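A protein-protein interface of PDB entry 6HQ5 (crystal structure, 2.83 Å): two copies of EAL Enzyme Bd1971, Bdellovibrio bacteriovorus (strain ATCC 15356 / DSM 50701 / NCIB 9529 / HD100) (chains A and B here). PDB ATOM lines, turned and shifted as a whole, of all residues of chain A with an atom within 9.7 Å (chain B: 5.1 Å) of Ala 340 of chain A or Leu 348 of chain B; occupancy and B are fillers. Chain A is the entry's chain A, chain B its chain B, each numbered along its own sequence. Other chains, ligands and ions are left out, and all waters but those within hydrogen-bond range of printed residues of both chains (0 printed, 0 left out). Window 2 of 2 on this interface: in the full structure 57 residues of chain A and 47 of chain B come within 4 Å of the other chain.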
ATOM      1  N   PHE A 304       7.755 -27.110 -30.295  1.00  0.00           N
ATOM      2  CA  PHE A 304       8.697 -26.136 -29.725  1.00  0.00           C
ATOM      3  C   PHE A 304       8.598 -26.094 -28.201  1.00  0.00           C
ATOM      4  O   PHE A 304       7.500 -26.087 -27.649  1.00  0.00           O
ATOM      5  CB  PHE A 304       8.439 -24.738 -30.298  1.00  0.00           C
ATOM      6  CG  PHE A 304       9.351 -23.665 -29.747  1.00  0.00           C
ATOM      7  CD1 PHE A 304      10.632 -23.484 -30.258  1.00  0.00           C
ATOM      8  CD2 PHE A 304       8.923 -22.823 -28.727  1.00  0.00           C
ATOM      9  CE1 PHE A 304      11.466 -22.497 -29.754  1.00  0.00           C
ATOM     10  CE2 PHE A 304       9.754 -21.837 -28.219  1.00  0.00           C
ATOM     11  CZ  PHE A 304      11.027 -21.672 -28.733  1.00  0.00           C
ATOM     12  N   LEU A 311      16.305 -21.928 -27.940  1.00  0.00           N
ATOM     13  CA  LEU A 311      16.232 -20.499 -27.606  1.00  0.00           C
ATOM     14  C   LEU A 311      17.367 -19.726 -28.257  1.00  0.00           C
ATOM     15  O   LEU A 311      17.120 -18.765 -28.974  1.00  0.00           O
ATOM     16  CB  LEU A 311      16.260 -20.275 -26.089  1.00  0.00           C
ATOM     17  CG  LEU A 311      14.954 -20.469 -25.306  1.00  0.00           C
ATOM     18  CD1 LEU A 311      13.837 -19.593 -25.857  1.00  0.00           C
ATOM     19  CD2 LEU A 311      14.528 -21.933 -25.279  1.00  0.00           C
ATOM     20  N   ILE A 324       2.966 -23.676 -31.337  1.00  0.00           N
ATOM     21  CA  ILE A 324       2.705 -23.964 -29.927  1.00  0.00           C
ATOM     22  C   ILE A 324       2.025 -25.332 -29.877  1.00  0.00           C
ATOM     23  O   ILE A 324       0.915 -25.495 -30.372  1.00  0.00           O
ATOM     24  CB  ILE A 324       1.821 -22.896 -29.232  1.00  0.00           C
ATOM     25  CG1 ILE A 324       2.627 -21.629 -28.945  1.00  0.00           C
ATOM     26  CG2 ILE A 324       1.283 -23.412 -27.900  1.00  0.00           C
ATOM     27  CD1 ILE A 324       2.824 -20.746 -30.147  1.00  0.00           C
ATOM     28  N   PHE A 328       0.806 -27.756 -24.488  1.00  0.00           N
ATOM     29  CA  PHE A 328       0.602 -26.473 -23.816  1.00  0.00           C
ATOM     30  C   PHE A 328      -0.858 -26.038 -23.877  1.00  0.00           C
ATOM     31  O   PHE A 328      -1.446 -25.673 -22.859  1.00  0.00           O
ATOM     32  CB  PHE A 328       1.460 -25.375 -24.450  1.00  0.00           C
ATOM     33  CG  PHE A 328       2.934 -25.553 -24.240  1.00  0.00           C
ATOM     34  CD1 PHE A 328       3.489 -25.427 -22.974  1.00  0.00           C
ATOM     35  CD2 PHE A 328       3.774 -25.818 -25.314  1.00  0.00           C
ATOM     36  CE1 PHE A 328       4.849 -25.581 -22.777  1.00  0.00           C
ATOM     37  CE2 PHE A 328       5.135 -25.971 -25.124  1.00  0.00           C
ATOM     38  CZ  PHE A 328       5.674 -25.853 -23.855  1.00  0.00           C
ATOM     39  N   LYS A 331      -3.708 -27.409 -21.615  1.00  0.00           N
ATOM     40  CA  LYS A 331      -3.628 -26.996 -20.212  1.00  0.00           C
ATOM     41  C   LYS A 331      -3.670 -25.470 -20.027  1.00  0.00           C
ATOM     42  O   LYS A 331      -3.431 -24.969 -18.927  1.00  0.00           O
ATOM     43  CB  LYS A 331      -2.335 -27.521 -19.594  1.00  0.00           C
ATOM     44  CG  LYS A 331      -2.083 -29.036 -19.721  1.00  0.00           C
ATOM     45  CD  LYS A 331      -2.963 -29.928 -18.838  1.00  0.00           C
ATOM     46  CE  LYS A 331      -4.293 -30.319 -19.462  1.00  0.00           C
ATOM     47  NZ  LYS A 331      -5.417 -30.445 -18.490  1.00  0.00           N
ATOM     48  N   ILE A 332      -3.987 -24.732 -21.088  1.00  0.00           N
ATOM     49  CA  ILE A 332      -3.893 -23.272 -21.059  1.00  0.00           C
ATOM     50  C   ILE A 332      -4.906 -22.655 -20.091  1.00  0.00           C
ATOM     51  O   ILE A 332      -4.618 -21.651 -19.451  1.00  0.00           O
ATOM     52  CB  ILE A 332      -4.023 -22.666 -22.481  1.00  0.00           C
ATOM     53  CG1 ILE A 332      -3.376 -21.285 -22.543  1.00  0.00           C
ATOM     54  CG2 ILE A 332      -5.474 -22.596 -22.947  1.00  0.00           C
ATOM     55  CD1 ILE A 332      -3.363 -20.691 -23.936  1.00  0.00           C
ATOM     56  N   LEU A 333      -6.083 -23.266 -19.984  1.00  0.00           N
ATOM     57  CA  LEU A 333      -7.096 -22.855 -19.018  1.00  0.00           C
ATOM     58  C   LEU A 333      -6.923 -23.595 -17.692  1.00  0.00           C
ATOM     59  O   LEU A 333      -7.239 -23.055 -16.633  1.00  0.00           O
ATOM     60  CB  LEU A 333      -8.485 -23.140 -19.589  1.00  0.00           C
ATOM     61  CG  LEU A 333      -8.794 -22.443 -20.936  1.00  0.00           C
ATOM     62  CD1 LEU A 333     -10.075 -22.906 -21.625  1.00  0.00           C
ATOM     63  CD2 LEU A 333      -8.821 -20.932 -20.766  1.00  0.00           C
ATOM     64  N   ASP A 335      -4.140 -24.736 -15.798  1.00  0.00           N
ATOM     65  CA  ASP A 335      -3.272 -24.019 -14.857  1.00  0.00           C
ATOM     66  C   ASP A 335      -2.676 -22.769 -15.514  1.00  0.00           C
ATOM     67  O   ASP A 335      -2.416 -22.763 -16.722  1.00  0.00           O
ATOM     68  CB  ASP A 335      -2.171 -24.931 -14.293  1.00  0.00           C
ATOM     69  CG  ASP A 335      -1.167 -25.385 -15.342  1.00  0.00           C
ATOM     70  OD1 ASP A 335      -1.499 -25.421 -16.543  1.00  0.00           O
ATOM     71  OD2 ASP A 335      -0.026 -25.706 -14.955  1.00  0.00           O
ATOM     72  N   PRO A 336      -2.465 -21.703 -14.717  1.00  0.00           N
ATOM     73  CA  PRO A 336      -1.968 -20.435 -15.255  1.00  0.00           C
ATOM     74  C   PRO A 336      -0.471 -20.437 -15.579  1.00  0.00           C
ATOM     75  O   PRO A 336       0.005 -19.531 -16.268  1.00  0.00           O
ATOM     76  CB  PRO A 336      -2.267 -19.446 -14.128  1.00  0.00           C
ATOM     77  CG  PRO A 336      -2.165 -20.266 -12.889  1.00  0.00           C
ATOM     78  CD  PRO A 336      -2.641 -21.645 -13.252  1.00  0.00           C
ATOM     79  N   LYS A 337       0.261 -21.438 -15.091  1.00  0.00           N
ATOM     80  CA  LYS A 337       1.689 -21.554 -15.376  1.00  0.00           C
ATOM     81  C   LYS A 337       1.954 -21.738 -16.870  1.00  0.00           C
ATOM     82  O   LYS A 337       2.762 -21.014 -17.451  1.00  0.00           O
ATOM     83  CB  LYS A 337       2.312 -22.715 -14.596  1.00  0.00           C
ATOM     84  CG  LYS A 337       2.302 -22.537 -13.083  1.00  0.00           C
ATOM     85  CD  LYS A 337       3.465 -23.306 -12.437  1.00  0.00           C
ATOM     86  CE  LYS A 337       3.072 -24.717 -12.030  1.00  0.00           C
ATOM     87  NZ  LYS A 337       4.257 -25.523 -11.616  1.00  0.00           N
ATOM     88  N   SER A 338       1.266 -22.696 -17.490  1.00  0.00           N
ATOM     89  CA  SER A 338       1.439 -22.968 -18.924  1.00  0.00           C
ATOM     90  C   SER A 338       0.824 -21.884 -19.812  1.00  0.00           C
ATOM     91  O   SER A 338       1.196 -21.759 -20.977  1.00  0.00           O
ATOM     92  CB  SER A 338       0.871 -24.341 -19.294  1.00  0.00           C
ATOM     93  OG  SER A 338      -0.359 -24.572 -18.652  1.00  0.00           O
ATOM     94  N   LYS A 339      -0.113 -21.110 -19.269  1.00  0.00           N
ATOM     95  CA  LYS A 339      -0.635 -19.944 -19.975  1.00  0.00           C
ATOM     96  C   LYS A 339       0.440 -18.864 -20.099  1.00  0.00           C
ATOM     97  O   LYS A 339       0.561 -18.217 -21.142  1.00  0.00           O
ATOM     98  CB  LYS A 339      -1.858 -19.384 -19.253  1.00  0.00           C
ATOM     99  CG  LYS A 339      -2.517 -18.215 -19.966  1.00  0.00           C
ATOM    100  CD  LYS A 339      -3.740 -17.733 -19.209  1.00  0.00           C
ATOM    101  CE  LYS A 339      -4.308 -16.482 -19.846  1.00  0.00           C
ATOM    102  NZ  LYS A 339      -5.541 -15.997 -19.164  1.00  0.00           N
ATOM    103  N   ALA A 340       1.202 -18.665 -19.025  1.00  0.00           N
ATOM    104  CA  ALA A 340       2.305 -17.702 -19.017  1.00  0.00           C
ATOM    105  C   ALA A 340       3.349 -18.068 -20.064  1.00  0.00           C
ATOM    106  O   ALA A 340       3.837 -17.206 -20.796  1.00  0.00           O
ATOM    107  CB  ALA A 340       2.948 -17.642 -17.640  1.00  0.00           C
ATOM    108  N   VAL A 341       3.674 -19.354 -20.131  1.00  0.00           N
ATOM    109  CA  VAL A 341       4.646 -19.857 -21.093  1.00  0.00           C
ATOM    110  C   VAL A 341       4.177 -19.594 -22.524  1.00  0.00           C
ATOM    111  O   VAL A 341       4.968 -19.170 -23.365  1.00  0.00           O
ATOM    112  CB  VAL A 341       4.908 -21.363 -20.887  1.00  0.00           C
ATOM    113  CG1 VAL A 341       5.790 -21.922 -21.997  1.00  0.00           C
ATOM    114  CG2 VAL A 341       5.557 -21.605 -19.531  1.00  0.00           C
ATOM    115  N   VAL A 342       2.894 -19.830 -22.792  1.00  0.00           N
ATOM    116  CA  VAL A 342       2.334 -19.617 -24.130  1.00  0.00           C
ATOM    117  C   VAL A 342       2.377 -18.142 -24.504  1.00  0.00           C
ATOM    118  O   VAL A 342       2.744 -17.787 -25.624  1.00  0.00           O
ATOM    119  CB  VAL A 342       0.889 -20.148 -24.245  1.00  0.00           C
ATOM    120  CG1 VAL A 342       0.245 -19.703 -25.551  1.00  0.00           C
ATOM    121  CG2 VAL A 342       0.874 -21.670 -24.162  1.00  0.00           C
ATOM    122  N   SER A 343       2.012 -17.283 -23.560  1.00  0.00           N
ATOM    123  CA  SER A 343       2.105 -15.842 -23.770  1.00  0.00           C
ATOM    124  C   SER A 343       3.538 -15.453 -24.124  1.00  0.00           C
ATOM    125  O   SER A 343       3.774 -14.683 -25.060  1.00  0.00           O
ATOM    126  CB  SER A 343       1.658 -15.091 -22.518  1.00  0.00           C
ATOM    127  OG  SER A 343       1.612 -13.698 -22.770  1.00  0.00           O
ATOM    128  N   SER A 344       4.484 -16.013 -23.380  1.00  0.00           N
ATOM    129  CA  SER A 344       5.891 -15.715 -23.574  1.00  0.00           C
ATOM    130  C   SER A 344       6.369 -16.144 -24.957  1.00  0.00           C
ATOM    131  O   SER A 344       7.021 -15.375 -25.662  1.00  0.00           O
ATOM    132  CB  SER A 344       6.723 -16.407 -22.497  1.00  0.00           C
ATOM    133  OG  SER A 344       7.997 -15.809 -22.396  1.00  0.00           O
ATOM    134  N   ILE A 345       6.044 -17.377 -25.332  1.00  0.00           N
ATOM    135  CA  ILE A 345       6.419 -17.918 -26.639  1.00  0.00           C
ATOM    136  C   ILE A 345       5.903 -17.024 -27.765  1.00  0.00           C
ATOM    137  O   ILE A 345       6.645 -16.708 -28.695  1.00  0.00           O
ATOM    138  CB  ILE A 345       5.891 -19.361 -26.826  1.00  0.00           C
ATOM    139  CG1 ILE A 345       6.673 -20.331 -25.934  1.00  0.00           C
ATOM    140  CG2 ILE A 345       6.009 -19.805 -28.278  1.00  0.00           C
ATOM    141  CD1 ILE A 345       6.004 -21.677 -25.752  1.00  0.00           C
ATOM    142  N   ILE A 346       4.637 -16.623 -27.670  1.00  0.00           N
ATOM    143  CA  ILE A 346       3.988 -15.837 -28.725  1.00  0.00           C
ATOM    144  C   ILE A 346       4.670 -14.487 -28.918  1.00  0.00           C
ATOM    145  O   ILE A 346       4.945 -14.082 -30.053  1.00  0.00           O
ATOM    146  CB  ILE A 346       2.489 -15.608 -28.429  1.00  0.00           C
ATOM    147  CG1 ILE A 346       1.718 -16.925 -28.530  1.00  0.00           C
ATOM    148  CG2 ILE A 346       1.891 -14.595 -29.405  1.00  0.00           C
ATOM    149  CD1 ILE A 346       0.392 -16.915 -27.799  1.00  0.00           C
ATOM    150  N   HIS A 347       4.932 -13.797 -27.807  1.00  0.00           N
ATOM    151  CA  HIS A 347       5.556 -12.477 -27.853  1.00  0.00           C
ATOM    152  C   HIS A 347       7.002 -12.574 -28.323  1.00  0.00           C
ATOM    153  O   HIS A 347       7.449 -11.758 -29.126  1.00  0.00           O
ATOM    154  CB  HIS A 347       5.463 -11.774 -26.495  1.00  0.00           C
ATOM    155  CG  HIS A 347       4.088 -11.266 -26.178  1.00  0.00           C
ATOM    156  ND1 HIS A 347       3.248 -11.895 -25.284  1.00  0.00           N
ATOM    157  CD2 HIS A 347       3.403 -10.198 -26.650  1.00  0.00           C
ATOM    158  CE1 HIS A 347       2.108 -11.232 -25.214  1.00  0.00           C
ATOM    159  NE2 HIS A 347       2.175 -10.198 -26.033  1.00  0.00           N
ATOM    160  N   LEU A 348       7.720 -13.582 -27.833  1.00  0.00           N
ATOM    161  CA  LEU A 348       9.087 -13.830 -28.278  1.00  0.00           C
ATOM    162  C   LEU A 348       9.113 -14.012 -29.788  1.00  0.00           C
ATOM    163  O   LEU A 348       9.896 -13.363 -30.479  1.00  0.00           O
ATOM    164  CB  LEU A 348       9.663 -15.069 -27.594  1.00  0.00           C
ATOM    165  CG  LEU A 348      11.068 -15.490 -28.031  1.00  0.00           C
ATOM    166  CD1 LEU A 348      12.063 -14.357 -27.820  1.00  0.00           C
ATOM    167  CD2 LEU A 348      11.502 -16.751 -27.294  1.00  0.00           C
ATOM    168  N   VAL A 369      -8.709 -17.062 -26.007  1.00  0.00           N
ATOM    169  CA  VAL A 369      -7.544 -16.708 -25.199  1.00  0.00           C
ATOM    170  C   VAL A 369      -6.316 -16.545 -26.093  1.00  0.00           C
ATOM    171  O   VAL A 369      -5.614 -15.537 -26.017  1.00  0.00           O
ATOM    172  CB  VAL A 369      -7.274 -17.768 -24.104  1.00  0.00           C
ATOM    173  CG1 VAL A 369      -5.951 -17.504 -23.392  1.00  0.00           C
ATOM    174  CG2 VAL A 369      -8.416 -17.799 -23.098  1.00  0.00           C
ATOM    175  N   LEU A 370      -6.080 -17.537 -26.951  1.00  0.00           N
ATOM    176  CA  LEU A 370      -4.936 -17.527 -27.870  1.00  0.00           C
ATOM    177  C   LEU A 370      -4.974 -16.313 -28.795  1.00  0.00           C
ATOM    178  O   LEU A 370      -3.934 -15.747 -29.133  1.00  0.00           O
ATOM    179  CB  LEU A 370      -4.895 -18.821 -28.695  1.00  0.00           C
ATOM    180  CG  LEU A 370      -4.612 -20.098 -27.894  1.00  0.00           C
ATOM    181  CD1 LEU A 370      -5.043 -21.324 -28.681  1.00  0.00           C
ATOM    182  CD2 LEU A 370      -3.145 -20.199 -27.502  1.00  0.00           C
ATOM    183  N   LEU A 373      -3.990 -13.278 -26.786  1.00  0.00           N
ATOM    184  CA  LEU A 373      -2.551 -13.378 -26.519  1.00  0.00           C
ATOM    185  C   LEU A 373      -1.696 -13.031 -27.737  1.00  0.00           C
ATOM    186  O   LEU A 373      -0.503 -12.776 -27.596  1.00  0.00           O
ATOM    187  CB  LEU A 373      -2.166 -14.771 -25.994  1.00  0.00           C
ATOM    188  CG  LEU A 373      -2.197 -14.961 -24.478  1.00  0.00           C
ATOM    189  CD1 LEU A 373      -3.576 -14.683 -23.909  1.00  0.00           C
ATOM    190  CD2 LEU A 373      -1.707 -16.344 -24.067  1.00  0.00           C
ATOM    191  N   LEU B 311      10.939 -25.134 -21.649  1.00  0.00           N
ATOM    192  CA  LEU B 311       9.705 -24.366 -21.539  1.00  0.00           C
ATOM    193  C   LEU B 311       8.617 -25.176 -20.841  1.00  0.00           C
ATOM    194  O   LEU B 311       7.950 -24.692 -19.923  1.00  0.00           O
ATOM    195  CB  LEU B 311       9.227 -23.870 -22.904  1.00  0.00           C
ATOM    196  CG  LEU B 311       9.969 -22.666 -23.495  1.00  0.00           C
ATOM    197  CD1 LEU B 311       9.987 -21.480 -22.537  1.00  0.00           C
ATOM    198  CD2 LEU B 311      11.384 -23.035 -23.918  1.00  0.00           C
ATOM    199  N   LEU B 314       9.119 -25.865 -16.988  1.00  0.00           N
ATOM    200  CA  LEU B 314       8.748 -24.830 -16.025  1.00  0.00           C
ATOM    201  C   LEU B 314       7.314 -25.006 -15.562  1.00  0.00           C
ATOM    202  O   LEU B 314       6.923 -24.508 -14.507  1.00  0.00           O
ATOM    203  CB  LEU B 314       8.916 -23.445 -16.657  1.00  0.00           C
ATOM    204  CG  LEU B 314      10.290 -22.821 -16.510  1.00  0.00           C
ATOM    205  CD1 LEU B 314      11.327 -23.691 -17.191  1.00  0.00           C
ATOM    206  CD2 LEU B 314      10.325 -21.403 -17.061  1.00  0.00           C
ATOM    207  N   SER B 343      15.510 -10.653 -22.259  1.00  0.00           N
ATOM    208  CA  SER B 343      14.374  -9.922 -21.720  1.00  0.00           C
ATOM    209  C   SER B 343      13.203 -10.865 -21.498  1.00  0.00           C
ATOM    210  O   SER B 343      12.551 -10.832 -20.456  1.00  0.00           O
ATOM    211  CB  SER B 343      13.958  -8.805 -22.670  1.00  0.00           C
ATOM    212  OG  SER B 343      12.959  -7.992 -22.082  1.00  0.00           O
ATOM    213  N   SER B 344      12.958 -11.712 -22.492  1.00  0.00           N
ATOM    214  CA  SER B 344      11.848 -12.658 -22.459  1.00  0.00           C
ATOM    215  C   SER B 344      11.998 -13.650 -21.315  1.00  0.00           C
ATOM    216  O   SER B 344      11.063 -13.859 -20.545  1.00  0.00           O
ATOM    217  CB  SER B 344      11.756 -13.411 -23.782  1.00  0.00           C
ATOM    218  OG  SER B 344      10.484 -14.003 -23.918  1.00  0.00           O
ATOM    219  N   ILE B 345      13.184 -14.241 -21.203  1.00  0.00           N
ATOM    220  CA  ILE B 345      13.481 -15.189 -20.133  1.00  0.00           C
ATOM    221  C   ILE B 345      13.240 -14.565 -18.758  1.00  0.00           C
ATOM    222  O   ILE B 345      12.605 -15.181 -17.902  1.00  0.00           O
ATOM    223  CB  ILE B 345      14.935 -15.698 -20.224  1.00  0.00           C
ATOM    224  CG1 ILE B 345      15.099 -16.630 -21.428  1.00  0.00           C
ATOM    225  CG2 ILE B 345      15.333 -16.441 -18.953  1.00  0.00           C
ATOM    226  CD1 ILE B 345      16.539 -16.876 -21.826  1.00  0.00           C
ATOM    227  N   ILE B 346      13.738 -13.343 -18.560  1.00  0.00           N
ATOM    228  CA  ILE B 346      13.640 -12.654 -17.264  1.00  0.00           C
ATOM    229  C   ILE B 346      12.182 -12.412 -16.866  1.00  0.00           C
ATOM    230  O   ILE B 346      11.801 -12.670 -15.720  1.00  0.00           O
ATOM    231  CB  ILE B 346      14.397 -11.304 -17.265  1.00  0.00           C
ATOM    232  CG1 ILE B 346      15.906 -11.540 -17.364  1.00  0.00           C
ATOM    233  CG2 ILE B 346      14.091 -10.503 -15.999  1.00  0.00           C
ATOM    234  CD1 ILE B 346      16.684 -10.339 -17.856  1.00  0.00           C
ATOM    235  N   HIS B 347      11.384 -11.913 -17.809  1.00  0.00           N
ATOM    236  CA  HIS B 347       9.978 -11.609 -17.545  1.00  0.00           C
ATOM    237  C   HIS B 347       9.175 -12.882 -17.331  1.00  0.00           C
ATOM    238  O   HIS B 347       8.336 -12.945 -16.434  1.00  0.00           O
ATOM    239  CB  HIS B 347       9.374 -10.750 -18.664  1.00  0.00           C
ATOM    240  CG  HIS B 347       9.834  -9.324 -18.632  1.00  0.00           C
ATOM    241  ND1 HIS B 347      10.782  -8.825 -19.500  1.00  0.00           N
ATOM    242  CD2 HIS B 347       9.502  -8.299 -17.810  1.00  0.00           C
ATOM    243  CE1 HIS B 347      11.003  -7.551 -19.225  1.00  0.00           C
ATOM    244  NE2 HIS B 347      10.239  -7.208 -18.203  1.00  0.00           N
ATOM    245  N   LEU B 348       9.444 -13.895 -18.144  1.00  0.00           N
ATOM    246  CA  LEU B 348       8.804 -15.192 -17.975  1.00  0.00           C
ATOM    247  C   LEU B 348       9.067 -15.719 -16.574  1.00  0.00           C
ATOM    248  O   LEU B 348       8.140 -16.111 -15.874  1.00  0.00           O
ATOM    249  CB  LEU B 348       9.324 -16.190 -19.011  1.00  0.00           C
ATOM    250  CG  LEU B 348       8.796 -17.627 -18.911  1.00  0.00           C
ATOM    251  CD1 LEU B 348       7.275 -17.652 -18.982  1.00  0.00           C
ATOM    252  CD2 LEU B 348       9.404 -18.493 -20.006  1.00  0.00           C
ATOM    253  N   ALA B 349      10.340 -15.711 -16.177  1.00  0.00           N
ATOM    254  CA  ALA B 349      10.755 -16.156 -14.845  1.00  0.00           C
ATOM    255  C   ALA B 349       9.983 -15.449 -13.739  1.00  0.00           C
ATOM    256  O   ALA B 349       9.492 -16.094 -12.816  1.00  0.00           O
ATOM    257  CB  ALA B 349      12.250 -15.944 -14.658  1.00  0.00           C
ATOM    258  N   HIS B 350       9.865 -14.127 -13.840  1.00  0.00           N
ATOM    259  CA  HIS B 350       9.080 -13.363 -12.874  1.00  0.00           C
ATOM    260  C   HIS B 350       7.622 -13.832 -12.860  1.00  0.00           C
ATOM    261  O   HIS B 350       7.077 -14.132 -11.799  1.00  0.00           O
ATOM    262  CB  HIS B 350       9.154 -11.861 -13.162  1.00  0.00           C
ATOM    263  CG  HIS B 350      10.516 -11.267 -12.961  1.00  0.00           C
ATOM    264  ND1 HIS B 350      11.444 -11.796 -12.090  1.00  0.00           N
ATOM    265  CD2 HIS B 350      11.096 -10.171 -13.506  1.00  0.00           C
ATOM    266  CE1 HIS B 350      12.543 -11.062 -12.120  1.00  0.00           C
ATOM    267  NE2 HIS B 350      12.357 -10.068 -12.968  1.00  0.00           N
ATOM    268  N   ALA B 351       7.011 -13.928 -14.038  1.00  0.00           N
ATOM    269  CA  ALA B 351       5.635 -14.421 -14.165  1.00  0.00           C
ATOM    270  C   ALA B 351       5.430 -15.809 -13.535  1.00  0.00           C
ATOM    271  O   ALA B 351       4.375 -16.083 -12.970  1.00  0.00           O
ATOM    272  CB  ALA B 351       5.222 -14.446 -15.627  1.00  0.00           C
ATOM    273  N   MET B 352       6.441 -16.671 -13.629  1.00  0.00           N
ATOM    274  CA  MET B 352       6.417 -17.990 -12.984  1.00  0.00           C
ATOM    275  C   MET B 352       6.733 -17.924 -11.483  1.00  0.00           C
ATOM    276  O   MET B 352       6.718 -18.948 -10.802  1.00  0.00           O
ATOM    277  CB  MET B 352       7.443 -18.918 -13.644  1.00  0.00           C
ATOM    278  CG  MET B 352       7.256 -19.168 -15.135  1.00  0.00           C
ATOM    279  SD  MET B 352       5.719 -19.983 -15.584  1.00  0.00           S
ATOM    280  CE  MET B 352       5.677 -21.324 -14.407  1.00  0.00           C
ATOM    281  N   ASP B 353       7.022 -16.725 -10.975  1.00  0.00           N
ATOM    282  CA  ASP B 353       7.471 -16.514  -9.597  1.00  0.00           C
ATOM    283  C   ASP B 353       8.887 -17.037  -9.340  1.00  0.00           C
ATOM    284  O   ASP B 353       9.257 -17.307  -8.197  1.00  0.00           O
ATOM    285  CB  ASP B 353       6.487 -17.129  -8.588  1.00  0.00           C
ATOM    286  CG  ASP B 353       6.124 -16.166  -7.485  1.00  0.00           C
ATOM    287  OD1 ASP B 353       5.239 -15.317  -7.717  1.00  0.00           O
ATOM    288  OD2 ASP B 353       6.729 -16.253  -6.394  1.00  0.00           O
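Of the printed residues of chain B, Lys 337 of chain A touches Met 352.
Ala 340 of chain A touches just one residue of chain B: Leu 348.
Of the printed residues of chain B, Ser 344 of chain A touches Ser 344 and Leu 348.
Of the printed residues of chain A, Leu 311 of chain B touches Leu 311 (3.6 Å) and Val 341 (3.9 Å).
Leu 348 of chain B touches just these residues of chain A: Ala 340 and Ser 344.
Ala 349 of chain B touches none of the printed residues of chain A.
No residue of chain A comes within 4 Å of Ala 351 of chain B.
Printed residues of chain A within 4 Å of Met 352 of chain B: Lys 337 (3.6 Å).
The nearest residue of chain A that does not touch Leu 348 of chain B is Val 341 of chain A (4.03 Å).
Leu 311 of chain A touches Leu 311 of chain B (CD2 to CD2, 3.6 Å).
Ala 340 of chain A touches Leu 348 of chain B.
CG2 of Val 341 of chain A touches O of Leu 311 of chain B, 3.9 Å away.
Ser 344 of chain A touches Leu 348 of chain B.
Ser 344 of chain B touches Leu 348 of chain A (OG to CB, 3.9 Å).
The side-chain hydroxyl (OG) of Ser 344 of chain A is in hydrogen-bond range of the side-chain hydroxyl (OG) of Ser 344 of chain B (3.4 Å).
O of Lys 337 of chain A sits close to SD of Met 352 of chain B (3.6 Å).
Leu 311 of chain B touches its own counterpart, Leu 311 of chain A.
Ser 344 of chain B touches its own counterpart, Ser 344 of chain A.
Ser 344 of chain A touches Leu 348 of chain B, and with the chains exchanged Leu 348 of chain A touches Ser 344 of chain B.
Positions printed for both chains: 311, 343, 344, 345, 346, 347 and 348.
Of the 7 pairs that touch across the chains among the printed residues, 4 have their exchanged pair printed and touching as well.
Of the 13 printed residues of chain B, 4 touch a printed residue of chain A.
Of the 24 printed residues of chain A, 6 touch a printed residue of chain B.
Along chain A the printed residues that touch a printed residue of chain B span positions 311 to 348.
Among the printed residues, 7 pairs touch across the chains.
Among the printed residues, no Asp or Glu carboxylate lies within 4 Å of a Lys or Arg side-chain nitrogen of the other chain.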
